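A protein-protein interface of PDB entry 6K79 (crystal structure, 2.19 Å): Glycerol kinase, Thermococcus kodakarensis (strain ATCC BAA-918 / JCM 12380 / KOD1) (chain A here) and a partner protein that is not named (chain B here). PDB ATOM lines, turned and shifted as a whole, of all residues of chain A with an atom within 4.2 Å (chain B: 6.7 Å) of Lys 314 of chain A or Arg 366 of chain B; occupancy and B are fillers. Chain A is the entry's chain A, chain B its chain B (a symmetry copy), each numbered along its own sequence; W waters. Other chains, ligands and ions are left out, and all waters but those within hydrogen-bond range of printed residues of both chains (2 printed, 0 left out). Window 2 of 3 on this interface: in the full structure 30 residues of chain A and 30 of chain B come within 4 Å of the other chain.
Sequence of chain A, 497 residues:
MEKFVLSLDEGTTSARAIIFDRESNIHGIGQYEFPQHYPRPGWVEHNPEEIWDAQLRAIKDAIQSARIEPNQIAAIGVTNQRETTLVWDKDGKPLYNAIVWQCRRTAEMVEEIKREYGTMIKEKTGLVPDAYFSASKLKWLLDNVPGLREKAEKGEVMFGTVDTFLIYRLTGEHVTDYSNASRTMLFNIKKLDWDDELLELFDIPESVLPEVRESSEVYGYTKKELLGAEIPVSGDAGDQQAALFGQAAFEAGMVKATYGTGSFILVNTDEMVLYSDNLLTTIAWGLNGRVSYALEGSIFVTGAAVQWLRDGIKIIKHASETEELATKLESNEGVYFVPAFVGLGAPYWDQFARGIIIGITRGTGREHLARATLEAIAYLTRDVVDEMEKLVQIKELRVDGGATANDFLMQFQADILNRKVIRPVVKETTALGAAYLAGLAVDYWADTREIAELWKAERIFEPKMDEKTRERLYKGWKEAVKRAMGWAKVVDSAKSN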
ATOM      1  N   LEU A 309       2.298   8.976 -13.581  1.00  0.00           N
ATOM      2  CA  LEU A 309       2.914  10.209 -14.080  1.00  0.00           C
ATOM      3  C   LEU A 309       3.840  10.819 -13.015  1.00  0.00           C
ATOM      4  O   LEU A 309       4.875  11.394 -13.330  1.00  0.00           O
ATOM      5  CB  LEU A 309       1.837  11.233 -14.436  1.00  0.00           C
ATOM      6  CG  LEU A 309       0.918  10.918 -15.610  1.00  0.00           C
ATOM      7  CD1 LEU A 309       0.020  12.108 -15.880  1.00  0.00           C
ATOM      8  CD2 LEU A 309       1.705  10.552 -16.850  1.00  0.00           C
ATOM      9  N   ARG A 310       3.401  10.775 -11.778  1.00  0.00           N
ATOM     10  CA  ARG A 310       4.058  11.443 -10.697  1.00  0.00           C
ATOM     11  C   ARG A 310       5.261  10.625 -10.228  1.00  0.00           C
ATOM     12  O   ARG A 310       6.272  11.247  -9.935  1.00  0.00           O
ATOM     13  CB  ARG A 310       3.091  11.629  -9.523  1.00  0.00           C
ATOM     14  CG  ARG A 310       3.669  12.397  -8.339  1.00  0.00           C
ATOM     15  CD  ARG A 310       2.752  12.477  -7.120  1.00  0.00           C
ATOM     16  NE  ARG A 310       2.627  11.142  -6.540  1.00  0.00           N
ATOM     17  CZ  ARG A 310       1.536  10.648  -5.966  1.00  0.00           C
ATOM     18  NH1 ARG A 310       0.507  11.441  -5.712  1.00  0.00           N
ATOM     19  NH2 ARG A 310       1.485   9.364  -5.663  1.00  0.00           N
ATOM     20  N   ASP A 311       5.125   9.289 -10.103  1.00  0.00           N
ATOM     21  CA  ASP A 311       6.136   8.426  -9.405  1.00  0.00           C
ATOM     22  C   ASP A 311       6.861   7.447 -10.350  1.00  0.00           C
ATOM     23  O   ASP A 311       7.887   6.895  -9.956  1.00  0.00           O
ATOM     24  CB  ASP A 311       5.510   7.624  -8.252  1.00  0.00           C
ATOM     25  CG  ASP A 311       4.800   8.511  -7.239  1.00  0.00           C
ATOM     26  OD1 ASP A 311       5.176   9.690  -7.146  1.00  0.00           O
ATOM     27  OD2 ASP A 311       3.861   8.037  -6.560  1.00  0.00           O
ATOM     28  N   GLY A 312       6.356   7.162 -11.550  1.00  0.00           N
ATOM     29  CA  GLY A 312       7.087   6.286 -12.471  1.00  0.00           C
ATOM     30  C   GLY A 312       7.997   7.068 -13.418  1.00  0.00           C
ATOM     31  O   GLY A 312       9.224   6.856 -13.530  1.00  0.00           O
ATOM     32  N   ILE A 313       7.360   7.997 -14.099  1.00  0.00           N
ATOM     33  CA  ILE A 313       7.972   8.747 -15.161  1.00  0.00           C
ATOM     34  C   ILE A 313       8.343  10.165 -14.673  1.00  0.00           C
ATOM     35  O   ILE A 313       9.238  10.832 -15.236  1.00  0.00           O
ATOM     36  CB  ILE A 313       7.029   8.598 -16.372  1.00  0.00           C
ATOM     37  CG1 ILE A 313       7.854   8.173 -17.572  1.00  0.00           C
ATOM     38  CG2 ILE A 313       6.105   9.739 -16.687  1.00  0.00           C
ATOM     39  CD1 ILE A 313       8.294   6.753 -17.403  1.00  0.00           C
ATOM     40  N   LYS A 314       7.747  10.583 -13.554  1.00  0.00           N
ATOM     41  CA  LYS A 314       8.154  11.788 -12.803  1.00  0.00           C
ATOM     42  C   LYS A 314       8.096  13.031 -13.697  1.00  0.00           C
ATOM     43  O   LYS A 314       9.018  13.803 -13.803  1.00  0.00           O
ATOM     44  CB  LYS A 314       9.515  11.539 -12.163  1.00  0.00           C
ATOM     45  CG  LYS A 314       9.497  10.424 -11.135  1.00  0.00           C
ATOM     46  CD  LYS A 314      10.653  10.492 -10.177  1.00  0.00           C
ATOM     47  CE  LYS A 314      11.928   9.969 -10.784  1.00  0.00           C
ATOM     48  NZ  LYS A 314      11.830   8.513 -11.007  1.00  0.00           N
ATOM     49  N   ILE A 315       6.941  13.193 -14.287  1.00  0.00           N
ATOM     50  CA  ILE A 315       6.633  14.201 -15.250  1.00  0.00           C
ATOM     51  C   ILE A 315       5.785  15.285 -14.570  1.00  0.00           C
ATOM     52  O   ILE A 315       5.637  16.333 -15.143  1.00  0.00           O
ATOM     53  CB  ILE A 315       5.972  13.496 -16.458  1.00  0.00           C
ATOM     54  CG1 ILE A 315       6.812  13.708 -17.705  1.00  0.00           C
ATOM     55  CG2 ILE A 315       4.501  13.793 -16.715  1.00  0.00           C
ATOM     56  CD1 ILE A 315       8.042  12.864 -17.710  1.00  0.00           C
ATOM     57  N   ILE A 316       5.212  14.997 -13.385  1.00  0.00           N
ATOM     58  CA  ILE A 316       4.532  15.972 -12.530  1.00  0.00           C
ATOM     59  C   ILE A 316       5.062  15.749 -11.108  1.00  0.00           C
ATOM     60  O   ILE A 316       5.685  14.736 -10.831  1.00  0.00           O
ATOM     61  CB  ILE A 316       2.988  15.850 -12.601  1.00  0.00           C
ATOM     62  CG1 ILE A 316       2.513  14.432 -12.263  1.00  0.00           C
ATOM     63  CG2 ILE A 316       2.465  16.313 -13.950  1.00  0.00           C
ATOM     64  CD1 ILE A 316       1.022  14.258 -12.096  1.00  0.00           C
ATOM     65  N   ARG A 366       4.528  17.099 -22.064  1.00  0.00           N
ATOM     66  CA  ARG A 366       3.972  16.667 -20.791  1.00  0.00           C
ATOM     67  C   ARG A 366       2.473  17.008 -20.755  1.00  0.00           C
ATOM     68  O   ARG A 366       1.688  16.292 -20.148  1.00  0.00           O
ATOM     69  CB  ARG A 366       4.714  17.338 -19.632  1.00  0.00           C
ATOM     70  CG  ARG A 366       6.128  16.817 -19.414  1.00  0.00           C
ATOM     71  CD  ARG A 366       6.861  17.518 -18.270  1.00  0.00           C
ATOM     72  NE  ARG A 366       8.142  16.870 -17.967  1.00  0.00           N
ATOM     73  CZ  ARG A 366       8.841  17.061 -16.843  1.00  0.00           C
ATOM     74  NH1 ARG A 366       8.417  17.954 -15.961  1.00  0.00           N
ATOM     75  NH2 ARG A 366       9.945  16.372 -16.603  1.00  0.00           N
ATOM     76  N   LEU B 309      12.746  12.712 -25.838  1.00  0.00           N
ATOM     77  CA  LEU B 309      12.910  12.425 -24.412  1.00  0.00           C
ATOM     78  C   LEU B 309      13.407  13.675 -23.682  1.00  0.00           C
ATOM     79  O   LEU B 309      13.093  13.865 -22.506  1.00  0.00           O
ATOM     80  CB  LEU B 309      13.931  11.309 -24.171  1.00  0.00           C
ATOM     81  CG  LEU B 309      13.578   9.925 -24.720  1.00  0.00           C
ATOM     82  CD1 LEU B 309      14.667   8.939 -24.333  1.00  0.00           C
ATOM     83  CD2 LEU B 309      12.222   9.466 -24.215  1.00  0.00           C
ATOM     84  N   ILE B 313       8.905  15.236 -23.430  1.00  0.00           N
ATOM     85  CA  ILE B 313       8.419  14.789 -22.112  1.00  0.00           C
ATOM     86  C   ILE B 313       9.442  15.119 -21.011  1.00  0.00           C
ATOM     87  O   ILE B 313       9.076  15.078 -19.808  1.00  0.00           O
ATOM     88  CB  ILE B 313       8.024  13.301 -22.129  1.00  0.00           C
ATOM     89  CG1 ILE B 313       9.197  12.368 -22.429  1.00  0.00           C
ATOM     90  CG2 ILE B 313       6.890  13.095 -23.111  1.00  0.00           C
ATOM     91  CD1 ILE B 313       8.900  10.937 -22.063  1.00  0.00           C
ATOM     92  N   LYS B 314      10.687  15.410 -21.418  1.00  0.00           N
ATOM     93  CA  LYS B 314      11.719  15.976 -20.568  1.00  0.00           C
ATOM     94  C   LYS B 314      12.060  15.027 -19.428  1.00  0.00           C
ATOM     95  O   LYS B 314      12.113  15.436 -18.291  1.00  0.00           O
ATOM     96  CB  LYS B 314      11.306  17.341 -20.005  1.00  0.00           C
ATOM     97  CG  LYS B 314      11.197  18.440 -21.054  1.00  0.00           C
ATOM     98  CD  LYS B 314      10.402  19.644 -20.586  1.00  0.00           C
ATOM     99  CE  LYS B 314      10.358  20.722 -21.639  1.00  0.00           C
ATOM    100  NZ  LYS B 314       9.027  21.360 -21.664  1.00  0.00           N
ATOM    101  N   ILE B 315      12.345  13.783 -19.740  1.00  0.00           N
ATOM    102  CA  ILE B 315      12.764  12.846 -18.708  1.00  0.00           C
ATOM    103  C   ILE B 315      14.308  12.712 -18.676  1.00  0.00           C
ATOM    104  O   ILE B 315      14.815  11.982 -17.854  1.00  0.00           O
ATOM    105  CB  ILE B 315      12.075  11.481 -18.892  1.00  0.00           C
ATOM    106  CG1 ILE B 315      12.419  10.817 -20.218  1.00  0.00           C
ATOM    107  CG2 ILE B 315      10.578  11.592 -18.716  1.00  0.00           C
ATOM    108  CD1 ILE B 315      12.209   9.344 -20.205  1.00  0.00           C
ATOM    109  N   ILE B 316      15.056  13.414 -19.522  1.00  0.00           N
ATOM    110  CA  ILE B 316      16.537  13.463 -19.441  1.00  0.00           C
ATOM    111  C   ILE B 316      16.978  14.914 -19.680  1.00  0.00           C
ATOM    112  O   ILE B 316      16.244  15.647 -20.296  1.00  0.00           O
ATOM    113  CB  ILE B 316      17.166  12.528 -20.498  1.00  0.00           C
ATOM    114  CG1 ILE B 316      16.659  12.862 -21.903  1.00  0.00           C
ATOM    115  CG2 ILE B 316      16.900  11.079 -20.150  1.00  0.00           C
ATOM    116  CD1 ILE B 316      17.483  12.281 -23.022  1.00  0.00           C
ATOM    117  N   GLU B 321      22.636  10.802 -21.101  1.00  0.00           N
ATOM    118  CA  GLU B 321      22.001  10.168 -19.921  1.00  0.00           C
ATOM    119  C   GLU B 321      21.206   8.924 -20.338  1.00  0.00           C
ATOM    120  O   GLU B 321      20.915   8.061 -19.505  1.00  0.00           O
ATOM    121  CB  GLU B 321      21.018  11.103 -19.225  1.00  0.00           C
ATOM    122  CG  GLU B 321      21.638  12.383 -18.728  1.00  0.00           C
ATOM    123  CD  GLU B 321      20.640  13.388 -18.172  1.00  0.00           C
ATOM    124  OE1 GLU B 321      19.603  12.975 -17.616  1.00  0.00           O
ATOM    125  OE2 GLU B 321      20.908  14.587 -18.299  1.00  0.00           O
ATOM    126  N   LEU B 325      20.623   5.305 -17.949  1.00  0.00           N
ATOM    127  CA  LEU B 325      19.257   4.880 -17.613  1.00  0.00           C
ATOM    128  C   LEU B 325      18.974   3.478 -18.180  1.00  0.00           C
ATOM    129  O   LEU B 325      18.445   2.618 -17.490  1.00  0.00           O
ATOM    130  CB  LEU B 325      18.256   5.909 -18.154  1.00  0.00           C
ATOM    131  CG  LEU B 325      18.155   7.242 -17.398  1.00  0.00           C
ATOM    132  CD1 LEU B 325      17.237   8.214 -18.140  1.00  0.00           C
ATOM    133  CD2 LEU B 325      17.632   7.035 -15.986  1.00  0.00           C
ATOM    134  N   ALA B 326      19.329   3.257 -19.438  1.00  0.00           N
ATOM    135  CA  ALA B 326      19.061   2.021 -20.141  1.00  0.00           C
ATOM    136  C   ALA B 326      19.857   0.850 -19.553  1.00  0.00           C
ATOM    137  O   ALA B 326      19.355  -0.288 -19.556  1.00  0.00           O
ATOM    138  CB  ALA B 326      19.374   2.193 -21.599  1.00  0.00           C
ATOM    139  N   LEU B 329      18.800  -1.713 -16.507  1.00  0.00           N
ATOM    140  CA  LEU B 329      17.887  -2.791 -16.793  1.00  0.00           C
ATOM    141  C   LEU B 329      18.643  -3.893 -17.535  1.00  0.00           C
ATOM    142  O   LEU B 329      19.500  -3.610 -18.396  1.00  0.00           O
ATOM    143  CB  LEU B 329      16.765  -2.258 -17.692  1.00  0.00           C
ATOM    144  CG  LEU B 329      15.821  -1.211 -17.088  1.00  0.00           C
ATOM    145  CD1 LEU B 329      14.810  -0.726 -18.119  1.00  0.00           C
ATOM    146  CD2 LEU B 329      15.093  -1.775 -15.876  1.00  0.00           C
ATOM    147  N   THR B 364       6.834   0.933 -14.781  1.00  0.00           N
ATOM    148  CA  THR B 364       7.566   1.480 -15.902  1.00  0.00           C
ATOM    149  C   THR B 364       8.229   2.793 -15.471  1.00  0.00           C
ATOM    150  O   THR B 364       7.541   3.712 -15.011  1.00  0.00           O
ATOM    151  CB  THR B 364       6.654   1.711 -17.108  1.00  0.00           C
ATOM    152  OG1 THR B 364       6.024   0.492 -17.480  1.00  0.00           O
ATOM    153  CG2 THR B 364       7.407   2.256 -18.298  1.00  0.00           C
ATOM    154  N   GLY B 365       9.536   2.909 -15.656  1.00  0.00           N
ATOM    155  CA  GLY B 365      10.248   4.128 -15.236  1.00  0.00           C
ATOM    156  C   GLY B 365      10.891   4.871 -16.409  1.00  0.00           C
ATOM    157  O   GLY B 365      10.783   4.473 -17.587  1.00  0.00           O
ATOM    158  N   ARG B 366      11.596   5.936 -16.079  1.00  0.00           N
ATOM    159  CA  ARG B 366      12.434   6.614 -17.025  1.00  0.00           C
ATOM    160  C   ARG B 366      13.396   5.638 -17.709  1.00  0.00           C
ATOM    161  O   ARG B 366      13.683   5.807 -18.882  1.00  0.00           O
ATOM    162  CB  ARG B 366      13.225   7.717 -16.315  1.00  0.00           C
ATOM    163  CG  ARG B 366      12.336   8.842 -15.800  1.00  0.00           C
ATOM    164  CD  ARG B 366      13.111  10.095 -15.424  1.00  0.00           C
ATOM    165  NE  ARG B 366      12.169  11.185 -15.238  1.00  0.00           N
ATOM    166  CZ  ARG B 366      12.500  12.445 -15.014  1.00  0.00           C
ATOM    167  NH1 ARG B 366      13.779  12.766 -14.850  1.00  0.00           N
ATOM    168  NH2 ARG B 366      11.538  13.360 -14.987  1.00  0.00           N
ATOM    169  N   GLU B 367      13.892   4.656 -16.958  1.00  0.00           N
ATOM    170  CA  GLU B 367      14.848   3.662 -17.474  1.00  0.00           C
ATOM    171  C   GLU B 367      14.262   2.913 -18.676  1.00  0.00           C
ATOM    172  O   GLU B 367      14.967   2.688 -19.667  1.00  0.00           O
ATOM    173  CB  GLU B 367      15.204   2.607 -16.430  1.00  0.00           C
ATOM    174  CG  GLU B 367      15.915   3.173 -15.237  1.00  0.00           C
ATOM    175  CD  GLU B 367      14.983   3.659 -14.125  1.00  0.00           C
ATOM    176  OE1 GLU B 367      13.717   3.800 -14.364  1.00  0.00           O
ATOM    177  OE2 GLU B 367      15.529   3.918 -13.022  1.00  0.00           O
ATOM    178  N   HIS B 368      13.000   2.506 -18.549  1.00  0.00           N
ATOM    179  CA  HIS B 368      12.318   1.736 -19.596  1.00  0.00           C
ATOM    180  C   HIS B 368      12.183   2.594 -20.841  1.00  0.00           C
ATOM    181  O   HIS B 368      12.425   2.131 -21.945  1.00  0.00           O
ATOM    182  CB  HIS B 368      10.930   1.229 -19.135  1.00  0.00           C
ATOM    183  CG  HIS B 368      11.020   0.260 -18.016  1.00  0.00           C
ATOM    184  ND1 HIS B 368      11.118   0.669 -16.691  1.00  0.00           N
ATOM    185  CD2 HIS B 368      11.124  -1.089 -18.004  1.00  0.00           C
ATOM    186  CE1 HIS B 368      11.266  -0.391 -15.907  1.00  0.00           C
ATOM    187  NE2 HIS B 368      11.246  -1.485 -16.688  1.00  0.00           N
ATOM    188  N   LEU B 369      11.779   3.837 -20.647  1.00  0.00           N
ATOM    189  CA  LEU B 369      11.609   4.725 -21.808  1.00  0.00           C
ATOM    190  C   LEU B 369      12.973   4.977 -22.482  1.00  0.00           C
ATOM    191  O   LEU B 369      13.034   5.040 -23.693  1.00  0.00           O
ATOM    192  CB  LEU B 369      10.979   6.055 -21.374  1.00  0.00           C
ATOM    193  CG  LEU B 369       9.466   6.136 -21.509  1.00  0.00           C
ATOM    194  CD1 LEU B 369       8.808   4.885 -20.965  1.00  0.00           C
ATOM    195  CD2 LEU B 369       8.910   7.370 -20.818  1.00  0.00           C
ATOM    196  N   ALA B 370      14.029   5.191 -21.718  1.00  0.00           N
ATOM    197  CA  ALA B 370      15.303   5.458 -22.339  1.00  0.00           C
ATOM    198  C   ALA B 370      15.749   4.222 -23.107  1.00  0.00           C
ATOM    199  O   ALA B 370      16.190   4.320 -24.253  1.00  0.00           O
ATOM    200  CB  ALA B 370      16.344   5.855 -21.315  1.00  0.00           C
ATOM    201  N   ARG B 371      15.613   3.065 -22.471  1.00  0.00           N
ATOM    202  CA  ARG B 371      16.090   1.821 -23.106  1.00  0.00           C
ATOM    203  C   ARG B 371      15.256   1.525 -24.356  1.00  0.00           C
ATOM    204  O   ARG B 371      15.804   1.215 -25.388  1.00  0.00           O
ATOM    205  CB  ARG B 371      16.050   0.682 -22.094  1.00  0.00           C
ATOM    206  CG  ARG B 371      16.273  -0.692 -22.691  1.00  0.00           C
ATOM    207  CD  ARG B 371      16.913  -1.603 -21.677  1.00  0.00           C
ATOM    208  NE  ARG B 371      17.224  -2.816 -22.367  1.00  0.00           N
ATOM    209  CZ  ARG B 371      18.255  -3.577 -22.120  1.00  0.00           C
ATOM    210  NH1 ARG B 371      19.009  -3.372 -21.050  1.00  0.00           N
ATOM    211  NH2 ARG B 371      18.507  -4.528 -22.983  1.00  0.00           N
HETATM  212  O   HOH W   1       6.152  19.465 -21.876  1.00  0.00           O
HETATM  213  O   HOH W   2      12.270   6.290 -13.457  1.00  0.00           O
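Printed residues of chain A that touch a printed residue of chain B: Gly 312, Ile 313, Lys 314, Ile 315 and Arg 366.
Hydrophobic or aromatic side chains of chain A within 4 Å of the printed part of chain B: Ile 313 and Ile 315.
Of the 17 printed residues of chain B, 7 touch a printed residue of chain A.
Among the printed residues, no Asp or Glu carboxylate lies within 4 Å of a Lys or Arg side-chain nitrogen of the other chain.
Thr 364 of chain B touches Gly 312 of chain A.
O of Gly 312 of chain A touches CA of Gly 365 of chain B, at 3.4 Å.
Gly 312 of chain A touches Arg 366 of chain B (O to N, 3.6 Å).
Ile 313 of chain A touches Ile 315 of chain B (O to CG2, 3.8 Å).
CD1 of Ile 313 of chain A touches O of Thr 364 of chain B, at 3.9 Å.
Ile 313 of chain A touches Gly 365 of chain B.
Leu 369 of chain B touches Ile 313 of chain A (CD2 to CG1, 3.5 Å).
Ile 313 of chain B touches Ile 315 of chain A (O to CD1, 3.2 Å).
Ile 315 of chain B touches Ile 315 of chain A.
Arg 366 of chain B touches Arg 366 of chain A (NH2 to NH2, 3.8 Å).
The backbone carbonyl oxygen of Ile 313 of chain B lies within hydrogen-bond range of the guanidinium group of Arg 366 of chain A, at 2.7 Å.
O of Lys 314 of chain B lies within hydrogen-bond range of NH2 of Arg 366 of chain A, 2.9 Å away.
The backbone carbonyl oxygen (O) of Ile 313 of chain A is in hydrogen-bond range of the guanidinium group (NE) of Arg 366 of chain B, 3.0 Å away.
The guanidinium group (NH2) of Arg 366 of chain B lies within hydrogen-bond range of the backbone carbonyl oxygen (O) of Lys 314 of chain A (2.8 Å).
Water W2 lies within hydrogen-bond range of N of Arg 366 of chain B (2.7 Å), OE1 of Glu 367 of chain B (3.0 Å), O of Gly 312 of chain A (3.1 Å) and NZ of Lys 314 of chain A (3.3 Å).
Water W1 lies within hydrogen-bond range of the backbone NH (N) of Arg 366 of chain A and the side-chain amino group (NZ) of Lys 314 of chain B.
O of Leu 309 of chain B sits at hydrogen-bond distance from N of Lys 314 of chain B (3.1 Å).
The backbone carbonyl oxygen of Leu 309 of chain B is in hydrogen-bond range of the backbone NH of Ile 315 of chain B (2.9 Å).
The guanidinium group (NH1) of Arg 366 of chain B is in hydrogen-bond range of the backbone carbonyl oxygen (O) of Ile 315 of chain B (3.3 Å).
The backbone carbonyl oxygen (O) of Leu 309 of chain A is in hydrogen-bond range of the backbone NH (N) of Lys 314 of chain A.
O of Leu 309 of chain A is in hydrogen-bond range of N of Ile 315 of chain A (2.9 Å).
The backbone carbonyl oxygen (O) of Ile 315 of chain A is in hydrogen-bond range of the guanidinium group (NH1) of Arg 366 of chain A, 3.3 Å away.
Of the printed residues of chain B, Gly 312 of chain A touches Thr 364, Gly 365 and Arg 366.
Printed residues of chain B within 4 Å of Ile 313 of chain A: Ile 315 (3.8 Å), Thr 364 (3.9 Å), Gly 365 (3.4 Å), Arg 366 (3.0 Å) and Leu 369 (3.5 Å).
Lys 314 of chain A touches just one residue of chain B: Arg 366.
Of the printed residues of chain B, Ile 315 of chain A touches Ile 313 (3.2 Å) and Ile 315 (3.0 Å).
Printed residues of chain A within 4 Å of Thr 364 of chain B: Gly 312 and Ile 313.
The nearest residue of chain B that does not touch Lys 314 of chain A is Ile 315 of chain B (5.6 Å).
The nearest printed residue of chain A that does not touch Thr 364 of chain B is Asp 311 of chain A (6.0 Å).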
